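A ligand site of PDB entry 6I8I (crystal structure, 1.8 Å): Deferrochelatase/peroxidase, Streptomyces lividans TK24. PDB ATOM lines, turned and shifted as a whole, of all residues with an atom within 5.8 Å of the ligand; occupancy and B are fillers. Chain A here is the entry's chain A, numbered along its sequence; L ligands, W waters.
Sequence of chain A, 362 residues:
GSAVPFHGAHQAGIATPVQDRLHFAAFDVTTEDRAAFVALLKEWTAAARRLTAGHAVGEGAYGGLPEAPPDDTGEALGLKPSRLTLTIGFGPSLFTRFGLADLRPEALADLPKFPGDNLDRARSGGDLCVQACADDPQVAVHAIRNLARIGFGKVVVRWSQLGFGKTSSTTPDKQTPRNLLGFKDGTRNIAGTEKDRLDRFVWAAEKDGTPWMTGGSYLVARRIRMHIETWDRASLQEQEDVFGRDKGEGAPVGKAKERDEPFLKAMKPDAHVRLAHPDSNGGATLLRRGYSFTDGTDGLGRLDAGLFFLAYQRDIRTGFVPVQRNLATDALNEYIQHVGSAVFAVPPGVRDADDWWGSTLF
N of Thr 187 lies within hydrogen-bond range of O1 of the ligand (3.3 Å).
The backbone NH (N) of Gly 186 lies within hydrogen-bond range of an oxygen (O1) of the ligand (2.7 Å).
An iron atom (FE1) of the ligand is bound by a ring nitrogen (NE2) of His 272.
N of Arg 188 is in hydrogen-bond range of O2 of the ligand, 3.0 Å away.
O3 of the ligand is in salt-bridge range of NE of Arg 188 (2.6 Å).
The guanidinium group (NH2) of Arg 288 is in salt-bridge range of an oxygen (O1) of the ligand (2.8 Å).
The side-chain amide oxygen (OD1) of Asn 179 sits at hydrogen-bond distance from the backbone NH (N) of Leu 181, at 3.0 Å.
The backbone carbonyl oxygen (O) of Arg 188 lies within hydrogen-bond range of the guanidinium group (NH2) of Arg 288 (3.0 Å).
OD1 of Asn 189 is in hydrogen-bond range of N of Arg 288, 2.8 Å away.
N of Leu 307 sits at hydrogen-bond distance from O of Ile 224 (2.8 Å).
The guanidinium group (NH1) of Arg 288 lies within salt-bridge range of the side-chain carboxylate (OD1) of Asp 185 (3.1 Å).
The backbone NH of Val 273 is in hydrogen-bond range of the backbone carbonyl oxygen of Phe 243.
The side-chain amide oxygen (OD1) of Asn 179 is in hydrogen-bond range of the backbone NH (N) of Phe 183, 3.4 Å away.
The guanidinium group (NH1) of Arg 188 sits at hydrogen-bond distance from a ring nitrogen (NE2) of His 277 (3.4 Å).
Asn 179 touches the ligand (ND2 to C17, 3.5 Å).
Leu 181 touches the ligand.
Phe 183 touches the ligand (CB to C9, 3.8 Å).
Lys 184 touches the ligand (O to C9, 3.2 Å).
Asp 185 touches the ligand.
Ile 224 touches the ligand (CG2 to C19, 3.97 Å).
CE of Met 226 touches C19 of the ligand, at 3.6 Å.
Phe 243 touches the ligand (CE1 to C2, 3.4 Å).
Arg 245 touches the ligand (NE to C10, 3.8 Å).
Val 273 touches the ligand.
Ala 276 touches the ligand.
His 277 touches the ligand.
Pro 278 touches the ligand (CD to O4, 3.0 Å).
CD1 of Leu 286 touches C25 of the ligand, at 3.95 Å.
Phe 309 touches the ligand.
CE1 of Phe 320 touches C26 of the ligand (3.4 Å).
Gln 324 touches the ligand (OE1 to C26, 3.6 Å).
Leu 332 touches the ligand (CD2 to C15, 3.7 Å).
Ile 336 touches the ligand (CG2 to C19, 3.8 Å).
Within 4 Å of the ligand: Asn 179, Leu 181, Phe 183, Lys 184, Asp 185, Gly 186, Thr 187, Arg 188, Ile 224, Met 226, Phe 243, Arg 245, His 272, Val 273, Ala 276, His 277, Pro 278, Leu 286, Arg 288, Phe 309, Phe 320, Gln 324, Leu 332 and Ile 336.
Water W4 bridges an oxygen (O4) of the ligand (2.7 Å) and the backbone carbonyl oxygen (O) of Arg 188 (2.8 Å).
Water W3 bridges NH2 of Arg 245 (2.6 Å) and O2 of the ligand (2.7 Å).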
ATOM      1  N   ASN A 179      21.792  38.483  21.102  1.00  0.00           N
ATOM      2  CA  ASN A 179      20.340  38.458  21.098  1.00  0.00           C
ATOM      3  C   ASN A 179      19.826  38.661  22.536  1.00  0.00           C
ATOM      4  O   ASN A 179      20.599  38.877  23.472  1.00  0.00           O
ATOM      5  CB  ASN A 179      19.834  37.152  20.497  1.00  0.00           C
ATOM      6  CG  ASN A 179      20.427  35.934  21.178  1.00  0.00           C
ATOM      7  OD1 ASN A 179      20.484  35.864  22.422  1.00  0.00           O
ATOM      8  ND2 ASN A 179      20.902  34.981  20.390  1.00  0.00           N
ATOM      9  N   LEU A 181      18.578  36.660  24.647  1.00  0.00           N
ATOM     10  CA  LEU A 181      19.026  35.676  25.621  1.00  0.00           C
ATOM     11  C   LEU A 181      20.418  35.982  26.146  1.00  0.00           C
ATOM     12  O   LEU A 181      20.900  35.263  27.027  1.00  0.00           O
ATOM     13  CB  LEU A 181      18.994  34.285  24.989  1.00  0.00           C
ATOM     14  CG  LEU A 181      17.658  33.857  24.369  1.00  0.00           C
ATOM     15  CD1 LEU A 181      17.668  32.366  23.981  1.00  0.00           C
ATOM     16  CD2 LEU A 181      16.519  34.149  25.319  1.00  0.00           C
ATOM     17  N   PHE A 183      23.305  35.859  24.386  1.00  0.00           N
ATOM     18  CA  PHE A 183      24.399  35.200  23.696  1.00  0.00           C
ATOM     19  C   PHE A 183      24.754  35.904  22.396  1.00  0.00           C
ATOM     20  O   PHE A 183      23.881  36.442  21.708  1.00  0.00           O
ATOM     21  CB  PHE A 183      24.074  33.737  23.399  1.00  0.00           C
ATOM     22  CG  PHE A 183      24.260  32.828  24.570  1.00  0.00           C
ATOM     23  CD1 PHE A 183      23.335  32.817  25.621  1.00  0.00           C
ATOM     24  CD2 PHE A 183      25.345  31.971  24.638  1.00  0.00           C
ATOM     25  CE1 PHE A 183      23.511  31.966  26.704  1.00  0.00           C
ATOM     26  CE2 PHE A 183      25.521  31.120  25.721  1.00  0.00           C
ATOM     27  CZ  PHE A 183      24.600  31.122  26.760  1.00  0.00           C
ATOM     28  N   LYS A 184      26.041  35.898  22.061  1.00  0.00           N
ATOM     29  CA  LYS A 184      26.472  36.373  20.749  1.00  0.00           C
ATOM     30  C   LYS A 184      25.788  35.554  19.667  1.00  0.00           C
ATOM     31  O   LYS A 184      25.705  34.331  19.747  1.00  0.00           O
ATOM     32  CB  LYS A 184      27.985  36.274  20.594  1.00  0.00           C
ATOM     33  CG  LYS A 184      28.775  37.175  21.522  1.00  0.00           C
ATOM     34  CD  LYS A 184      30.269  36.955  21.305  1.00  0.00           C
ATOM     35  CE  LYS A 184      31.100  37.904  22.160  1.00  0.00           C
ATOM     36  NZ  LYS A 184      32.549  37.575  22.098  1.00  0.00           N
ATOM     37  N   ASP A 185      25.315  36.239  18.636  1.00  0.00           N
ATOM     38  CA  ASP A 185      24.527  35.620  17.593  1.00  0.00           C
ATOM     39  C   ASP A 185      25.111  36.069  16.266  1.00  0.00           C
ATOM     40  O   ASP A 185      24.985  37.244  15.903  1.00  0.00           O
ATOM     41  CB  ASP A 185      23.045  36.018  17.710  1.00  0.00           C
ATOM     42  CG  ASP A 185      22.079  34.940  17.203  1.00  0.00           C
ATOM     43  OD1 ASP A 185      22.431  34.204  16.253  1.00  0.00           O
ATOM     44  OD2 ASP A 185      20.965  34.848  17.753  1.00  0.00           O
ATOM     45  N   GLY A 186      25.719  35.151  15.523  1.00  0.00           N
ATOM     46  CA  GLY A 186      26.229  35.489  14.214  1.00  0.00           C
ATOM     47  C   GLY A 186      27.674  35.096  13.973  1.00  0.00           C
ATOM     48  O   GLY A 186      28.211  35.333  12.891  1.00  0.00           O
ATOM     49  N   THR A 187      28.322  34.466  14.954  1.00  0.00           N
ATOM     50  CA  THR A 187      29.743  34.118  14.816  1.00  0.00           C
ATOM     51  C   THR A 187      30.003  33.303  13.555  1.00  0.00           C
ATOM     52  O   THR A 187      30.786  33.705  12.689  1.00  0.00           O
ATOM     53  CB  THR A 187      30.208  33.367  16.056  1.00  0.00           C
ATOM     54  OG1 THR A 187      29.863  34.134  17.205  1.00  0.00           O
ATOM     55  CG2 THR A 187      31.736  33.176  16.018  1.00  0.00           C
ATOM     56  N   ARG A 188      29.347  32.150  13.423  1.00  0.00           N
ATOM     57  CA  ARG A 188      29.573  31.263  12.274  1.00  0.00           C
ATOM     58  C   ARG A 188      28.433  31.446  11.276  1.00  0.00           C
ATOM     59  O   ARG A 188      27.496  30.649  11.190  1.00  0.00           O
ATOM     60  CB  ARG A 188      29.739  29.810  12.718  1.00  0.00           C
ATOM     61  CG  ARG A 188      31.156  29.557  13.317  1.00  0.00           C
ATOM     62  CD  ARG A 188      31.412  28.055  13.544  1.00  0.00           C
ATOM     63  NE  ARG A 188      30.624  27.268  12.610  1.00  0.00           N
ATOM     64  CZ  ARG A 188      31.040  26.915  11.404  1.00  0.00           C
ATOM     65  NH1 ARG A 188      30.234  26.223  10.605  1.00  0.00           N
ATOM     66  NH2 ARG A 188      32.269  27.232  11.006  1.00  0.00           N
ATOM     67  N   ASN A 189      28.510  32.542  10.545  1.00  0.00           N
ATOM     68  CA  ASN A 189      27.585  32.884   9.468  1.00  0.00           C
ATOM     69  C   ASN A 189      28.408  33.000   8.191  1.00  0.00           C
ATOM     70  O   ASN A 189      29.620  32.777   8.184  1.00  0.00           O
ATOM     71  CB  ASN A 189      26.864  34.202   9.801  1.00  0.00           C
ATOM     72  CG  ASN A 189      25.542  34.347   9.065  1.00  0.00           C
ATOM     73  OD1 ASN A 189      24.795  33.393   8.905  1.00  0.00           O
ATOM     74  ND2 ASN A 189      25.234  35.580   8.644  1.00  0.00           N
ATOM     75  N   ILE A 224       9.769  34.582  16.131  1.00  0.00           N
ATOM     76  CA  ILE A 224      10.027  33.626  17.216  1.00  0.00           C
ATOM     77  C   ILE A 224       9.897  34.326  18.569  1.00  0.00           C
ATOM     78  O   ILE A 224      10.697  35.212  18.887  1.00  0.00           O
ATOM     79  CB  ILE A 224      11.398  32.968  17.080  1.00  0.00           C
ATOM     80  CG1 ILE A 224      11.523  32.277  15.719  1.00  0.00           C
ATOM     81  CG2 ILE A 224      11.599  31.953  18.211  1.00  0.00           C
ATOM     82  CD1 ILE A 224      12.940  31.738  15.438  1.00  0.00           C
ATOM     83  N   MET A 226      10.354  34.461  22.554  1.00  0.00           N
ATOM     84  CA  MET A 226      11.225  33.886  23.575  1.00  0.00           C
ATOM     85  C   MET A 226      10.514  33.880  24.927  1.00  0.00           C
ATOM     86  O   MET A 226       9.898  34.886  25.310  1.00  0.00           O
ATOM     87  CB  MET A 226      12.535  34.663  23.673  1.00  0.00           C
ATOM     88  CG  MET A 226      13.331  34.692  22.380  1.00  0.00           C
ATOM     89  SD  MET A 226      14.668  35.884  22.602  1.00  0.00           S
ATOM     90  CE  MET A 226      15.684  35.438  21.203  1.00  0.00           C
ATOM     91  N   PHE A 243      23.238  25.931  24.302  1.00  0.00           N
ATOM     92  CA  PHE A 243      23.829  26.404  23.058  1.00  0.00           C
ATOM     93  C   PHE A 243      25.063  25.632  22.645  1.00  0.00           C
ATOM     94  O   PHE A 243      25.241  25.356  21.462  1.00  0.00           O
ATOM     95  CB  PHE A 243      24.162  27.900  23.155  1.00  0.00           C
ATOM     96  CG  PHE A 243      22.947  28.779  22.991  1.00  0.00           C
ATOM     97  CD1 PHE A 243      22.270  28.822  21.765  1.00  0.00           C
ATOM     98  CD2 PHE A 243      22.486  29.552  24.039  1.00  0.00           C
ATOM     99  CE1 PHE A 243      21.133  29.625  21.617  1.00  0.00           C
ATOM    100  CE2 PHE A 243      21.358  30.357  23.888  1.00  0.00           C
ATOM    101  CZ  PHE A 243      20.689  30.390  22.680  1.00  0.00           C
ATOM    102  N   ARG A 245      28.065  26.959  23.626  1.00  0.00           N
ATOM    103  CA  ARG A 245      29.090  27.977  23.768  1.00  0.00           C
ATOM    104  C   ARG A 245      28.899  28.632  25.127  1.00  0.00           C
ATOM    105  O   ARG A 245      27.803  28.646  25.686  1.00  0.00           O
ATOM    106  CB  ARG A 245      29.010  29.028  22.644  1.00  0.00           C
ATOM    107  CG  ARG A 245      29.214  28.506  21.223  1.00  0.00           C
ATOM    108  CD  ARG A 245      29.093  29.649  20.220  1.00  0.00           C
ATOM    109  NE  ARG A 245      29.369  29.262  18.836  1.00  0.00           N
ATOM    110  CZ  ARG A 245      30.540  29.468  18.211  1.00  0.00           C
ATOM    111  NH1 ARG A 245      31.534  30.043  18.855  1.00  0.00           N
ATOM    112  NH2 ARG A 245      30.690  29.113  16.939  1.00  0.00           N
ATOM    113  N   PRO A 262      34.223  25.060  16.652  1.00  0.00           N
ATOM    114  CA  PRO A 262      33.558  24.160  17.599  1.00  0.00           C
ATOM    115  C   PRO A 262      34.047  22.735  17.404  1.00  0.00           C
ATOM    116  O   PRO A 262      34.328  22.300  16.289  1.00  0.00           O
ATOM    117  CB  PRO A 262      32.072  24.317  17.268  1.00  0.00           C
ATOM    118  CG  PRO A 262      32.033  24.880  15.892  1.00  0.00           C
ATOM    119  CD  PRO A 262      33.276  25.710  15.731  1.00  0.00           C
ATOM    120  N   HIS A 272      22.124  23.431  20.627  1.00  0.00           N
ATOM    121  CA  HIS A 272      21.691  24.144  19.427  1.00  0.00           C
ATOM    122  C   HIS A 272      22.783  24.195  18.360  1.00  0.00           C
ATOM    123  O   HIS A 272      22.534  23.862  17.209  1.00  0.00           O
ATOM    124  CB  HIS A 272      21.255  25.549  19.825  1.00  0.00           C
ATOM    125  CG  HIS A 272      20.712  26.354  18.694  1.00  0.00           C
ATOM    126  ND1 HIS A 272      19.515  26.060  18.080  1.00  0.00           N
ATOM    127  CD2 HIS A 272      21.213  27.432  18.044  1.00  0.00           C
ATOM    128  CE1 HIS A 272      19.293  26.929  17.116  1.00  0.00           C
ATOM    129  NE2 HIS A 272      20.311  27.768  17.075  1.00  0.00           N
ATOM    130  N   VAL A 273      23.999  24.601  18.732  1.00  0.00           N
ATOM    131  CA  VAL A 273      25.073  24.731  17.746  1.00  0.00           C
ATOM    132  C   VAL A 273      25.397  23.365  17.144  1.00  0.00           C
ATOM    133  O   VAL A 273      25.649  23.241  15.945  1.00  0.00           O
ATOM    134  CB  VAL A 273      26.311  25.383  18.373  1.00  0.00           C
ATOM    135  CG1 VAL A 273      27.545  25.155  17.512  1.00  0.00           C
ATOM    136  CG2 VAL A 273      26.067  26.876  18.549  1.00  0.00           C
ATOM    137  N   ALA A 276      22.557  22.604  14.590  1.00  0.00           N
ATOM    138  CA  ALA A 276      22.448  23.525  13.470  1.00  0.00           C
ATOM    139  C   ALA A 276      23.672  23.545  12.570  1.00  0.00           C
ATOM    140  O   ALA A 276      23.610  24.093  11.472  1.00  0.00           O
ATOM    141  CB  ALA A 276      22.178  24.945  13.974  1.00  0.00           C
ATOM    142  N   HIS A 277      24.768  22.939  13.010  1.00  0.00           N
ATOM    143  CA  HIS A 277      26.051  23.072  12.338  1.00  0.00           C
ATOM    144  C   HIS A 277      25.993  22.404  10.959  1.00  0.00           C
ATOM    145  O   HIS A 277      25.356  21.361  10.804  1.00  0.00           O
ATOM    146  CB  HIS A 277      27.139  22.429  13.197  1.00  0.00           C
ATOM    147  CG  HIS A 277      28.534  22.735  12.769  1.00  0.00           C
ATOM    148  ND1 HIS A 277      29.130  22.141  11.678  1.00  0.00           N
ATOM    149  CD2 HIS A 277      29.466  23.578  13.287  1.00  0.00           C
ATOM    150  CE1 HIS A 277      30.351  22.605  11.529  1.00  0.00           C
ATOM    151  NE2 HIS A 277      30.581  23.479  12.499  1.00  0.00           N
ATOM    152  N   PRO A 278      26.619  22.994   9.938  1.00  0.00           N
ATOM    153  CA  PRO A 278      26.649  22.340   8.617  1.00  0.00           C
ATOM    154  C   PRO A 278      27.055  20.871   8.654  1.00  0.00           C
ATOM    155  O   PRO A 278      26.437  20.057   7.950  1.00  0.00           O
ATOM    156  CB  PRO A 278      27.653  23.204   7.849  1.00  0.00           C
ATOM    157  CG  PRO A 278      27.396  24.585   8.359  1.00  0.00           C
ATOM    158  CD  PRO A 278      27.020  24.414   9.834  1.00  0.00           C
ATOM    159  N   LEU A 286      23.481  28.463   5.953  1.00  0.00           N
ATOM    160  CA  LEU A 286      22.516  29.544   5.869  1.00  0.00           C
ATOM    161  C   LEU A 286      23.231  30.881   6.033  1.00  0.00           C
ATOM    162  O   LEU A 286      24.246  30.961   6.724  1.00  0.00           O
ATOM    163  CB  LEU A 286      21.444  29.453   6.971  1.00  0.00           C
ATOM    164  CG  LEU A 286      20.624  28.177   6.977  1.00  0.00           C
ATOM    165  CD1 LEU A 286      19.700  28.170   8.184  1.00  0.00           C
ATOM    166  CD2 LEU A 286      19.839  28.091   5.673  1.00  0.00           C
ATOM    167  N   ARG A 288      22.174  33.949   7.970  1.00  0.00           N
ATOM    168  CA  ARG A 288      21.223  34.478   8.925  1.00  0.00           C
ATOM    169  C   ARG A 288      21.349  35.993   8.991  1.00  0.00           C
ATOM    170  O   ARG A 288      22.466  36.532   8.991  1.00  0.00           O
ATOM    171  CB  ARG A 288      21.459  33.857  10.302  1.00  0.00           C
ATOM    172  CG  ARG A 288      21.188  32.369  10.354  1.00  0.00           C
ATOM    173  CD  ARG A 288      21.641  31.751  11.666  1.00  0.00           C
ATOM    174  NE  ARG A 288      23.100  31.658  11.736  1.00  0.00           N
ATOM    175  CZ  ARG A 288      23.842  31.976  12.801  1.00  0.00           C
ATOM    176  NH1 ARG A 288      23.268  32.418  13.911  1.00  0.00           N
ATOM    177  NH2 ARG A 288      25.156  31.834  12.735  1.00  0.00           N
ATOM    178  N   LEU A 307      12.702  37.200  18.565  1.00  0.00           N
ATOM    179  CA  LEU A 307      13.702  37.309  17.527  1.00  0.00           C
ATOM    180  C   LEU A 307      12.995  37.140  16.197  1.00  0.00           C
ATOM    181  O   LEU A 307      12.233  36.185  16.021  1.00  0.00           O
ATOM    182  CB  LEU A 307      14.799  36.236  17.708  1.00  0.00           C
ATOM    183  CG  LEU A 307      16.037  36.373  16.809  1.00  0.00           C
ATOM    184  CD1 LEU A 307      17.243  35.706  17.464  1.00  0.00           C
ATOM    185  CD2 LEU A 307      15.796  35.756  15.435  1.00  0.00           C
ATOM    186  N   PHE A 309      13.593  36.088  12.860  1.00  0.00           N
ATOM    187  CA  PHE A 309      14.623  35.297  12.205  1.00  0.00           C
ATOM    188  C   PHE A 309      14.480  35.388  10.684  1.00  0.00           C
ATOM    189  O   PHE A 309      13.417  35.066  10.134  1.00  0.00           O
ATOM    190  CB  PHE A 309      14.523  33.851  12.698  1.00  0.00           C
ATOM    191  CG  PHE A 309      15.532  32.928  12.076  1.00  0.00           C
ATOM    192  CD1 PHE A 309      15.246  32.281  10.891  1.00  0.00           C
ATOM    193  CD2 PHE A 309      16.756  32.692  12.691  1.00  0.00           C
ATOM    194  CE1 PHE A 309      16.165  31.407  10.298  1.00  0.00           C
ATOM    195  CE2 PHE A 309      17.690  31.820  12.113  1.00  0.00           C
ATOM    196  CZ  PHE A 309      17.387  31.181  10.914  1.00  0.00           C
ATOM    197  N   PHE A 320      17.038  26.043   4.821  1.00  0.00           N
ATOM    198  CA  PHE A 320      16.290  26.152   6.074  1.00  0.00           C
ATOM    199  C   PHE A 320      15.634  24.831   6.457  1.00  0.00           C
ATOM    200  O   PHE A 320      15.668  24.424   7.622  1.00  0.00           O
ATOM    201  CB  PHE A 320      15.247  27.260   5.963  1.00  0.00           C
ATOM    202  CG  PHE A 320      14.370  27.376   7.182  1.00  0.00           C
ATOM    203  CD1 PHE A 320      14.796  28.094   8.285  1.00  0.00           C
ATOM    204  CD2 PHE A 320      13.125  26.763   7.227  1.00  0.00           C
ATOM    205  CE1 PHE A 320      13.993  28.204   9.419  1.00  0.00           C
ATOM    206  CE2 PHE A 320      12.318  26.873   8.352  1.00  0.00           C
ATOM    207  CZ  PHE A 320      12.744  27.582   9.444  1.00  0.00           C
ATOM    208  N   VAL A 323      17.864  22.060   8.203  1.00  0.00           N
ATOM    209  CA  VAL A 323      18.384  22.500   9.496  1.00  0.00           C
ATOM    210  C   VAL A 323      17.241  22.588  10.512  1.00  0.00           C
ATOM    211  O   VAL A 323      17.371  22.104  11.644  1.00  0.00           O
ATOM    212  CB  VAL A 323      19.132  23.835   9.368  1.00  0.00           C
ATOM    213  CG1 VAL A 323      19.714  24.221  10.714  1.00  0.00           C
ATOM    214  CG2 VAL A 323      20.250  23.756   8.308  1.00  0.00           C
ATOM    215  N   GLN A 324      16.109  23.181  10.124  1.00  0.00           N
ATOM    216  CA  GLN A 324      15.005  23.254  11.075  1.00  0.00           C
ATOM    217  C   GLN A 324      14.441  21.868  11.386  1.00  0.00           C
ATOM    218  O   GLN A 324      13.938  21.647  12.489  1.00  0.00           O
ATOM    219  CB  GLN A 324      13.908  24.179  10.544  1.00  0.00           C
ATOM    220  CG  GLN A 324      12.645  24.258  11.396  1.00  0.00           C
ATOM    221  CD  GLN A 324      12.806  24.952  12.745  1.00  0.00           C
ATOM    222  OE1 GLN A 324      13.604  25.866  12.898  1.00  0.00           O
ATOM    223  NE2 GLN A 324      12.017  24.526  13.717  1.00  0.00           N
ATOM    224  N   LEU A 327      16.415  20.497  14.144  1.00  0.00           N
ATOM    225  CA  LEU A 327      16.212  21.170  15.403  1.00  0.00           C
ATOM    226  C   LEU A 327      15.024  20.625  16.186  1.00  0.00           C
ATOM    227  O   LEU A 327      14.653  21.193  17.219  1.00  0.00           O
ATOM    228  CB  LEU A 327      16.032  22.679  15.184  1.00  0.00           C
ATOM    229  CG  LEU A 327      17.216  23.404  14.544  1.00  0.00           C
ATOM    230  CD1 LEU A 327      17.014  24.904  14.646  1.00  0.00           C
ATOM    231  CD2 LEU A 327      18.513  23.002  15.225  1.00  0.00           C
ATOM    232  N   LEU A 332      17.042  24.326  22.816  1.00  0.00           N
ATOM    233  CA  LEU A 332      16.479  25.666  22.789  1.00  0.00           C
ATOM    234  C   LEU A 332      14.959  25.663  22.723  1.00  0.00           C
ATOM    235  O   LEU A 332      14.310  26.623  23.177  1.00  0.00           O
ATOM    236  CB  LEU A 332      17.039  26.445  21.598  1.00  0.00           C
ATOM    237  CG  LEU A 332      16.672  27.912  21.475  1.00  0.00           C
ATOM    238  CD1 LEU A 332      17.017  28.654  22.761  1.00  0.00           C
ATOM    239  CD2 LEU A 332      17.389  28.509  20.292  1.00  0.00           C
ATOM    240  N   ILE A 336      11.525  28.825  23.267  1.00  0.00           N
ATOM    241  CA  ILE A 336      11.109  29.627  22.130  1.00  0.00           C
ATOM    242  C   ILE A 336       9.861  29.001  21.528  1.00  0.00           C
ATOM    243  O   ILE A 336       9.541  27.833  21.764  1.00  0.00           O
ATOM    244  CB  ILE A 336      12.200  29.732  21.033  1.00  0.00           C
ATOM    245  CG1 ILE A 336      12.500  28.339  20.436  1.00  0.00           C
ATOM    246  CG2 ILE A 336      13.438  30.404  21.566  1.00  0.00           C
ATOM    247  CD1 ILE A 336      13.347  28.389  19.150  1.00  0.00           C
ATOM    248  N   HIS A 338       7.760  29.363  17.555  1.00  0.00           N
ATOM    249  CA  HIS A 338       7.618  29.997  16.255  1.00  0.00           C
ATOM    250  C   HIS A 338       6.158  30.400  16.083  1.00  0.00           C
ATOM    251  O   HIS A 338       5.274  29.539  16.125  1.00  0.00           O
ATOM    252  CB  HIS A 338       8.035  29.058  15.130  1.00  0.00           C
ATOM    253  CG  HIS A 338       9.504  28.762  15.094  1.00  0.00           C
ATOM    254  ND1 HIS A 338      10.302  29.067  14.010  1.00  0.00           N
ATOM    255  CD2 HIS A 338      10.311  28.194  16.010  1.00  0.00           C
ATOM    256  CE1 HIS A 338      11.543  28.689  14.260  1.00  0.00           C
ATOM    257  NE2 HIS A 338      11.577  28.155  15.461  1.00  0.00           N
HETATM  258  C1  LIG L   1      24.144  29.479  15.754  1.00  0.00           C
HETATM  259  C2  LIG L   1      20.919  31.504  18.759  1.00  0.00           C
HETATM  260  C3  LIG L   1      17.280  30.101  15.918  1.00  0.00           C
HETATM  261  C4  LIG L   1      20.485  28.216  12.819  1.00  0.00           C
HETATM  262  C5  LIG L   1      23.595  30.125  16.833  1.00  0.00           C
HETATM  263  C6  LIG L   1      24.306  30.646  17.968  1.00  0.00           C
HETATM  264  C7  LIG L   1      23.409  31.191  18.792  1.00  0.00           C
HETATM  265  C8  LIG L   1      22.098  31.044  18.208  1.00  0.00           C
HETATM  266  C9  LIG L   1      23.688  31.881  20.137  1.00  0.00           C
HETATM  267  C10 LIG L   1      25.840  30.566  18.162  1.00  0.00           C
HETATM  268  C11 LIG L   1      26.586  31.731  17.505  1.00  0.00           C
HETATM  269  C12 LIG L   1      26.579  31.718  15.992  1.00  0.00           C
HETATM  270  O1  LIG L   1      25.756  32.445  15.380  1.00  0.00           O
HETATM  271  O2  LIG L   1      27.434  31.005  15.392  1.00  0.00           O
HETATM  272  C13 LIG L   1      19.647  31.326  18.245  1.00  0.00           C
HETATM  273  C14 LIG L   1      18.420  31.803  18.832  1.00  0.00           C
HETATM  274  C15 LIG L   1      17.404  31.403  18.044  1.00  0.00           C
HETATM  275  C16 LIG L   1      17.969  30.669  16.946  1.00  0.00           C
HETATM  276  C17 LIG L   1      18.356  32.616  20.138  1.00  0.00           C
HETATM  277  C18 LIG L   1      15.886  31.655  18.207  1.00  0.00           C
HETATM  278  C19 LIG L   1      15.426  32.515  19.112  1.00  0.00           C
HETATM  279  C20 LIG L   1      17.836  29.466  14.837  1.00  0.00           C
HETATM  280  C21 LIG L   1      17.096  28.871  13.759  1.00  0.00           C
HETATM  281  C22 LIG L   1      17.991  28.362  12.885  1.00  0.00           C
HETATM  282  C23 LIG L   1      19.304  28.599  13.409  1.00  0.00           C
HETATM  283  C24 LIG L   1      15.565  28.899  13.677  1.00  0.00           C
HETATM  284  C25 LIG L   1      17.739  27.603  11.571  1.00  0.00           C
HETATM  285  C26 LIG L   1      16.537  27.095  11.305  1.00  0.00           C
HETATM  286  C27 LIG L   1      21.734  28.439  13.331  1.00  0.00           C
HETATM  287  C28 LIG L   1      22.977  28.131  12.653  1.00  0.00           C
HETATM  288  C29 LIG L   1      23.984  28.455  13.451  1.00  0.00           C
HETATM  289  C30 LIG L   1      23.437  29.005  14.672  1.00  0.00           C
HETATM  290  C31 LIG L   1      23.117  27.500  11.248  1.00  0.00           C
HETATM  291  C32 LIG L   1      25.468  28.280  13.092  1.00  0.00           C
HETATM  292  C33 LIG L   1      26.036  27.010  13.715  1.00  0.00           C
HETATM  293  C34 LIG L   1      27.407  26.749  13.147  1.00  0.00           C
HETATM  294  O3  LIG L   1      28.397  26.764  13.916  1.00  0.00           O
HETATM  295  O4  LIG L   1      27.519  26.547  11.914  1.00  0.00           O
HETATM  296  N1  LIG L   1      22.242  30.390  17.020  1.00  0.00           N
HETATM  297  N2  LIG L   1      19.333  30.637  17.110  1.00  0.00           N
HETATM  298  N3  LIG L   1      19.187  29.279  14.601  1.00  0.00           N
HETATM  299  N4  LIG L   1      22.056  28.987  14.553  1.00  0.00           N
HETATM  300 FE1  LIG L   1      20.646  29.720  15.915  1.00  0.00          FE
HETATM  301  O   HOH W   1      24.751  27.766   8.542  1.00  0.00           O
HETATM  302  O   HOH W   2      23.643  25.355   8.922  1.00  0.00           O
HETATM  303  O   HOH W   3      28.283  28.608  16.251  1.00  0.00           O
HETATM  304  O   HOH W   4      27.168  28.195   9.861  1.00  0.00           O
